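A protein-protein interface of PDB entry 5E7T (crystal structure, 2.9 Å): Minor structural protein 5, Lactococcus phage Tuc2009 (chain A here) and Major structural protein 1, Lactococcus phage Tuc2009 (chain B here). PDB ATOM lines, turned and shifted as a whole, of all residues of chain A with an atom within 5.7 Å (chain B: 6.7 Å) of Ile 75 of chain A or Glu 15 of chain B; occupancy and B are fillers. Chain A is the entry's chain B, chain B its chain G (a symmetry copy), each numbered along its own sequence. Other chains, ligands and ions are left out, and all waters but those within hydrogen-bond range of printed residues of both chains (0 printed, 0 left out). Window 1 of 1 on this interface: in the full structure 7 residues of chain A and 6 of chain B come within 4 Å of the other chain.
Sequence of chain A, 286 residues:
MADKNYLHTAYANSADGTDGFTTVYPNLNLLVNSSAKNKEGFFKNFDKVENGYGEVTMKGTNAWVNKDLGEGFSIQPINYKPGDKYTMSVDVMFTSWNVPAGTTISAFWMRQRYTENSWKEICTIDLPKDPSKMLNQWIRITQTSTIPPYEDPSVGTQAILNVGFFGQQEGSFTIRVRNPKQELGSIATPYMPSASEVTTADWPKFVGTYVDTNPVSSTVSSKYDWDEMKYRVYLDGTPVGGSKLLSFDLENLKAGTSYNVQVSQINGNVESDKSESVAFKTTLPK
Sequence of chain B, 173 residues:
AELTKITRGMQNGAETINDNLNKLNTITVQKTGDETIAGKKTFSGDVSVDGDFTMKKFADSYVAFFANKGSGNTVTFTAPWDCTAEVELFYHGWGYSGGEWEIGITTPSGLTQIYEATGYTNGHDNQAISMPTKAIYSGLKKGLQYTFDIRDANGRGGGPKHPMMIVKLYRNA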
ATOM      1  N   LEU A  30      11.875 -16.536   7.596  1.00  0.00           N
ATOM      2  CA  LEU A  30      11.854 -16.034   8.971  1.00  0.00           C
ATOM      3  C   LEU A  30      12.764 -16.895   9.856  1.00  0.00           C
ATOM      4  O   LEU A  30      13.025 -16.524  10.984  1.00  0.00           O
ATOM      5  CB  LEU A  30      10.420 -15.952   9.502  1.00  0.00           C
ATOM      6  CG  LEU A  30       9.598 -14.822   8.912  1.00  0.00           C
ATOM      7  CD1 LEU A  30       8.133 -15.078   9.076  1.00  0.00           C
ATOM      8  CD2 LEU A  30       9.965 -13.530   9.533  1.00  0.00           C
ATOM      9  N   PHE A  73      14.660 -19.151  14.970  1.00  0.00           N
ATOM     10  CA  PHE A  73      13.490 -18.330  14.654  1.00  0.00           C
ATOM     11  C   PHE A  73      13.851 -16.863  14.841  1.00  0.00           C
ATOM     12  O   PHE A  73      14.206 -16.456  15.941  1.00  0.00           O
ATOM     13  CB  PHE A  73      12.245 -18.755  15.441  1.00  0.00           C
ATOM     14  CG  PHE A  73      11.586 -20.018  14.927  1.00  0.00           C
ATOM     15  CD1 PHE A  73      12.006 -21.266  15.361  1.00  0.00           C
ATOM     16  CD2 PHE A  73      10.523 -19.954  14.036  1.00  0.00           C
ATOM     17  CE1 PHE A  73      11.388 -22.432  14.898  1.00  0.00           C
ATOM     18  CE2 PHE A  73       9.894 -21.119  13.584  1.00  0.00           C
ATOM     19  CZ  PHE A  73      10.347 -22.355  14.002  1.00  0.00           C
ATOM     20  N   SER A  74      13.868 -16.105  13.723  1.00  0.00           N
ATOM     21  CA  SER A  74      14.235 -14.694  13.637  1.00  0.00           C
ATOM     22  C   SER A  74      13.621 -13.860  14.753  1.00  0.00           C
ATOM     23  O   SER A  74      14.324 -13.077  15.419  1.00  0.00           O
ATOM     24  CB  SER A  74      13.774 -14.121  12.304  1.00  0.00           C
ATOM     25  OG  SER A  74      14.855 -13.540  11.601  1.00  0.00           O
ATOM     26  N   ILE A  75      12.290 -14.031  14.934  1.00  0.00           N
ATOM     27  CA  ILE A  75      11.490 -13.271  15.882  1.00  0.00           C
ATOM     28  C   ILE A  75      10.520 -14.146  16.697  1.00  0.00           C
ATOM     29  O   ILE A  75       9.962 -15.130  16.199  1.00  0.00           O
ATOM     30  CB  ILE A  75      10.773 -12.105  15.150  1.00  0.00           C
ATOM     31  CG1 ILE A  75       9.966 -12.614  13.922  1.00  0.00           C
ATOM     32  CG2 ILE A  75      11.804 -11.004  14.770  1.00  0.00           C
ATOM     33  CD1 ILE A  75       8.923 -11.760  13.485  1.00  0.00           C
ATOM     34  N   GLN A  76      10.324 -13.744  17.954  1.00  0.00           N
ATOM     35  CA  GLN A  76       9.490 -14.415  18.930  1.00  0.00           C
ATOM     36  C   GLN A  76       8.049 -14.528  18.495  1.00  0.00           C
ATOM     37  O   GLN A  76       7.503 -13.558  17.972  1.00  0.00           O
ATOM     38  CB  GLN A  76       9.630 -13.751  20.299  1.00  0.00           C
ATOM     39  CG  GLN A  76      11.005 -13.963  20.933  1.00  0.00           C
ATOM     40  CD  GLN A  76      11.378 -15.417  20.982  1.00  0.00           C
ATOM     41  OE1 GLN A  76      10.733 -16.213  21.665  1.00  0.00           O
ATOM     42  NE2 GLN A  76      12.355 -15.808  20.167  1.00  0.00           N
ATOM     43  N   PRO A  77       7.422 -15.708  18.708  1.00  0.00           N
ATOM     44  CA  PRO A  77       6.058 -15.920  18.217  1.00  0.00           C
ATOM     45  C   PRO A  77       4.980 -15.024  18.806  1.00  0.00           C
ATOM     46  O   PRO A  77       3.894 -14.938  18.250  1.00  0.00           O
ATOM     47  CB  PRO A  77       5.805 -17.394  18.517  1.00  0.00           C
ATOM     48  CG  PRO A  77       6.755 -17.756  19.568  1.00  0.00           C
ATOM     49  CD  PRO A  77       7.962 -16.945  19.313  1.00  0.00           C
ATOM     50  N   ASN A  79       4.908 -11.973  18.559  1.00  0.00           N
ATOM     51  CA  ASN A  79       4.933 -10.793  17.715  1.00  0.00           C
ATOM     52  C   ASN A  79       4.001 -10.995  16.558  1.00  0.00           C
ATOM     53  O   ASN A  79       3.517 -10.016  15.995  1.00  0.00           O
ATOM     54  CB  ASN A  79       6.329 -10.519  17.221  1.00  0.00           C
ATOM     55  CG  ASN A  79       7.121  -9.683  18.168  1.00  0.00           C
ATOM     56  OD1 ASN A  79       6.881  -8.474  18.349  1.00  0.00           O
ATOM     57  ND2 ASN A  79       8.084 -10.314  18.781  1.00  0.00           N
ATOM     58  N   TYR A  80       3.727 -12.262  16.212  1.00  0.00           N
ATOM     59  CA  TYR A  80       2.803 -12.606  15.129  1.00  0.00           C
ATOM     60  C   TYR A  80       1.365 -12.182  15.559  1.00  0.00           C
ATOM     61  O   TYR A  80       1.005 -12.401  16.717  1.00  0.00           O
ATOM     62  CB  TYR A  80       2.868 -14.126  14.837  1.00  0.00           C
ATOM     63  CG  TYR A  80       4.236 -14.778  14.630  1.00  0.00           C
ATOM     64  CD1 TYR A  80       5.284 -14.080  14.037  1.00  0.00           C
ATOM     65  CD2 TYR A  80       4.426 -16.140  14.876  1.00  0.00           C
ATOM     66  CE1 TYR A  80       6.512 -14.697  13.775  1.00  0.00           C
ATOM     67  CE2 TYR A  80       5.635 -16.776  14.584  1.00  0.00           C
ATOM     68  CZ  TYR A  80       6.679 -16.051  14.037  1.00  0.00           C
ATOM     69  OH  TYR A  80       7.896 -16.656  13.792  1.00  0.00           O
ATOM     70  N   GLN A 112       6.492 -24.210  16.941  1.00  0.00           N
ATOM     71  CA  GLN A 112       6.545 -23.024  17.796  1.00  0.00           C
ATOM     72  C   GLN A 112       5.220 -23.134  18.535  1.00  0.00           C
ATOM     73  O   GLN A 112       4.180 -23.341  17.887  1.00  0.00           O
ATOM     74  CB  GLN A 112       6.552 -21.725  16.984  1.00  0.00           C
ATOM     75  CG  GLN A 112       7.914 -21.130  16.754  1.00  0.00           C
ATOM     76  CD  GLN A 112       7.817 -19.823  16.002  1.00  0.00           C
ATOM     77  OE1 GLN A 112       7.178 -19.735  14.945  1.00  0.00           O
ATOM     78  NE2 GLN A 112       8.526 -18.796  16.477  1.00  0.00           N
ATOM     79  N   ILE B   6      20.187  -4.017  15.608  1.00  0.00           N
ATOM     80  CA  ILE B   6      19.185  -3.129  15.004  1.00  0.00           C
ATOM     81  C   ILE B   6      19.945  -2.247  14.021  1.00  0.00           C
ATOM     82  O   ILE B   6      20.783  -1.441  14.439  1.00  0.00           O
ATOM     83  CB  ILE B   6      18.427  -2.282  16.075  1.00  0.00           C
ATOM     84  CG1 ILE B   6      17.758  -3.169  17.155  1.00  0.00           C
ATOM     85  CG2 ILE B   6      17.432  -1.317  15.439  1.00  0.00           C
ATOM     86  CD1 ILE B   6      16.833  -4.242  16.648  1.00  0.00           C
ATOM     87  N   GLN B  11      14.747  -5.635   8.149  1.00  0.00           N
ATOM     88  CA  GLN B  11      13.430  -6.220   8.121  1.00  0.00           C
ATOM     89  C   GLN B  11      13.179  -6.681   9.531  1.00  0.00           C
ATOM     90  O   GLN B  11      14.106  -7.096  10.237  1.00  0.00           O
ATOM     91  CB  GLN B  11      13.374  -7.413   7.157  1.00  0.00           C
ATOM     92  CG  GLN B  11      13.405  -7.024   5.686  1.00  0.00           C
ATOM     93  CD  GLN B  11      12.340  -6.044   5.284  1.00  0.00           C
ATOM     94  OE1 GLN B  11      11.138  -6.317   5.356  1.00  0.00           O
ATOM     95  NE2 GLN B  11      12.766  -4.875   4.866  1.00  0.00           N
ATOM     96  N   ASN B  12      11.927  -6.610   9.934  1.00  0.00           N
ATOM     97  CA  ASN B  12      11.442  -7.020  11.244  1.00  0.00           C
ATOM     98  C   ASN B  12      11.991  -6.164  12.361  1.00  0.00           C
ATOM     99  O   ASN B  12      12.252  -6.668  13.458  1.00  0.00           O
ATOM    100  CB  ASN B  12      11.684  -8.503  11.482  1.00  0.00           C
ATOM    101  CG  ASN B  12      11.164  -9.396  10.369  1.00  0.00           C
ATOM    102  OD1 ASN B  12       9.984  -9.327   9.954  1.00  0.00           O
ATOM    103  ND2 ASN B  12      12.038 -10.278   9.901  1.00  0.00           N
ATOM    104  N   GLY B  13      12.112  -4.865  12.079  1.00  0.00           N
ATOM    105  CA  GLY B  13      12.625  -3.856  12.998  1.00  0.00           C
ATOM    106  C   GLY B  13      11.845  -3.783  14.287  1.00  0.00           C
ATOM    107  O   GLY B  13      12.444  -3.878  15.349  1.00  0.00           O
ATOM    108  N   ALA B  14      10.499  -3.651  14.208  1.00  0.00           N
ATOM    109  CA  ALA B  14       9.628  -3.543  15.364  1.00  0.00           C
ATOM    110  C   ALA B  14       9.722  -4.763  16.251  1.00  0.00           C
ATOM    111  O   ALA B  14       9.889  -4.627  17.464  1.00  0.00           O
ATOM    112  CB  ALA B  14       8.198  -3.311  14.935  1.00  0.00           C
ATOM    113  N   GLU B  15       9.687  -5.954  15.665  1.00  0.00           N
ATOM    114  CA  GLU B  15       9.752  -7.201  16.443  1.00  0.00           C
ATOM    115  C   GLU B  15      11.118  -7.407  17.052  1.00  0.00           C
ATOM    116  O   GLU B  15      11.184  -7.802  18.219  1.00  0.00           O
ATOM    117  CB  GLU B  15       9.355  -8.415  15.611  1.00  0.00           C
ATOM    118  CG  GLU B  15       8.012  -8.253  14.938  1.00  0.00           C
ATOM    119  CD  GLU B  15       8.050  -7.692  13.543  1.00  0.00           C
ATOM    120  OE1 GLU B  15       8.954  -6.880  13.243  1.00  0.00           O
ATOM    121  OE2 GLU B  15       7.187  -8.090  12.732  1.00  0.00           O
ATOM    122  N   THR B  16      12.210  -7.107  16.285  1.00  0.00           N
ATOM    123  CA  THR B  16      13.556  -7.269  16.821  1.00  0.00           C
ATOM    124  C   THR B  16      13.772  -6.310  17.983  1.00  0.00           C
ATOM    125  O   THR B  16      14.329  -6.732  18.995  1.00  0.00           O
ATOM    126  CB  THR B  16      14.614  -7.193  15.729  1.00  0.00           C
ATOM    127  OG1 THR B  16      14.269  -8.048  14.628  1.00  0.00           O
ATOM    128  CG2 THR B  16      15.953  -7.595  16.220  1.00  0.00           C
ATOM    129  N   ILE B  17      13.265  -5.053  17.886  1.00  0.00           N
ATOM    130  CA  ILE B  17      13.355  -4.068  18.984  1.00  0.00           C
ATOM    131  C   ILE B  17      12.560  -4.617  20.189  1.00  0.00           C
ATOM    132  O   ILE B  17      13.060  -4.613  21.319  1.00  0.00           O
ATOM    133  CB  ILE B  17      12.908  -2.634  18.572  1.00  0.00           C
ATOM    134  CG1 ILE B  17      13.846  -2.040  17.522  1.00  0.00           C
ATOM    135  CG2 ILE B  17      12.859  -1.701  19.793  1.00  0.00           C
ATOM    136  CD1 ILE B  17      13.283  -0.896  16.773  1.00  0.00           C
ATOM    137  N   ASN B  18      11.355  -5.154  19.924  1.00  0.00           N
ATOM    138  CA  ASN B  18      10.498  -5.704  20.967  1.00  0.00           C
ATOM    139  C   ASN B  18      11.160  -6.851  21.679  1.00  0.00           C
ATOM    140  O   ASN B  18      11.158  -6.873  22.903  1.00  0.00           O
ATOM    141  CB  ASN B  18       9.168  -6.156  20.392  1.00  0.00           C
ATOM    142  CG  ASN B  18       8.074  -6.173  21.394  1.00  0.00           C
ATOM    143  OD1 ASN B  18       7.770  -5.160  22.014  1.00  0.00           O
ATOM    144  ND2 ASN B  18       7.407  -7.303  21.521  1.00  0.00           N
ATOM    145  N   ASP B  19      11.750  -7.789  20.919  1.00  0.00           N
ATOM    146  CA  ASP B  19      12.410  -8.965  21.469  1.00  0.00           C
ATOM    147  C   ASP B  19      13.604  -8.540  22.308  1.00  0.00           C
ATOM    148  O   ASP B  19      13.798  -9.079  23.398  1.00  0.00           O
ATOM    149  CB  ASP B  19      12.838  -9.942  20.359  1.00  0.00           C
ATOM    150  CG  ASP B  19      11.728 -10.656  19.592  1.00  0.00           C
ATOM    151  OD1 ASP B  19      10.569 -10.624  20.058  1.00  0.00           O
ATOM    152  OD2 ASP B  19      12.040 -11.301  18.548  1.00  0.00           O
ATOM    153  N   ASN B  20      14.369  -7.548  21.824  1.00  0.00           N
ATOM    154  CA  ASN B  20      15.544  -7.054  22.539  1.00  0.00           C
ATOM    155  C   ASN B  20      15.189  -6.369  23.865  1.00  0.00           C
ATOM    156  O   ASN B  20      15.858  -6.605  24.877  1.00  0.00           O
ATOM    157  CB  ASN B  20      16.393  -6.177  21.641  1.00  0.00           C
ATOM    158  CG  ASN B  20      17.061  -6.928  20.513  1.00  0.00           C
ATOM    159  OD1 ASN B  20      17.129  -8.161  20.461  1.00  0.00           O
ATOM    160  ND2 ASN B  20      17.576  -6.201  19.576  1.00  0.00           N
ATOM    161  N   ASN B  22      12.386  -7.025  25.507  1.00  0.00           N
ATOM    162  CA  ASN B  22      11.890  -8.126  26.326  1.00  0.00           C
ATOM    163  C   ASN B  22      13.041  -8.963  26.902  1.00  0.00           C
ATOM    164  O   ASN B  22      12.969  -9.332  28.066  1.00  0.00           O
ATOM    165  CB  ASN B  22      10.894  -8.975  25.554  1.00  0.00           C
ATOM    166  CG  ASN B  22       9.554  -8.317  25.305  1.00  0.00           C
ATOM    167  OD1 ASN B  22       9.131  -7.401  26.016  1.00  0.00           O
ATOM    168  ND2 ASN B  22       8.813  -8.822  24.323  1.00  0.00           N
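The side-chain carboxylate of Asp 19 of chain B sits at hydrogen-bond distance from the backbone NH of Gln 76 of chain A (3.0 Å). The side-chain carboxylate (OD1) of Asp 19 of chain B is in hydrogen-bond range of the side-chain amide nitrogen (ND2) of Asn 79 of chain A, 2.8 Å away. The side-chain amide nitrogen of Asn 18 of chain B is in hydrogen-bond range of the side-chain amide oxygen of Asn 79 of chain A, 3.4 Å away.
O of Asn 18 of chain B lies close to ND2 of Asn 22 of chain B, at 3.4 Å. The backbone carbonyl oxygen (O) of Leu 30 of chain A sits close to the backbone NH (N) of Ser 74 of chain A, at 2.9 Å. The backbone carbonyl oxygen of Gln 76 of chain A sits close to the side-chain amide nitrogen of Asn 79 of chain A (3.4 Å). The backbone carbonyl oxygen (O) of Asn 12 of chain B lies within hydrogen-bond range of the side-chain hydroxyl (OG1) of Thr 16 of chain B, at 2.7 Å. The side-chain amide nitrogen of Asn 20 of chain B sits close to the backbone carbonyl oxygen of Thr 16 of chain B, at 3.3 Å.
Among the printed residues, merely in contact across the chains: Ile 75 of chain A with Asp 19 of chain B, Asn 79 of chain A with Glu 15 of chain B, Ile 75 of chain A with Glu 15 of chain B, Ile 75 of chain A with Thr 16 of chain B and Leu 30 of chain A with Asn 12 of chain B.
Ile 75 of chain A touches just these residues of chain B: Glu 15 (3.7 Å), Thr 16 (3.9 Å) and Asp 19 (3.4 Å). Glu 15 of chain B touches just these residues of chain A: Ile 75 (3.7 Å) and Asn 79 (3.6 Å). Of the printed residues of chain A, Asp 19 of chain B touches Ile 75 (3.4 Å), Gln 76 (3.0 Å) and Asn 79 (2.8 Å). Of the printed residues of chain A, Asn 18 of chain B touches Asn 79. Of the printed residues of chain B, Asn 79 of chain A touches Glu 15, Asn 18 and Asp 19. Phe 73 of chain A touches none of the printed residues of chain B.
Of the 9 printed residues of chain A, 4 touch a printed residue of chain B. Of the 12 printed residues of chain B, 5 touch a printed residue of chain A. Printed residues of chain B that touch a printed residue of chain A: Asn 12, Glu 15, Thr 16, Asn 18 and Asp 19. Among the printed residues, 8 pairs touch across the chains. Among the printed residues, no Asp or Glu carboxylate lies within 4 Å of a Lys or Arg side-chain nitrogen of the other chain.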
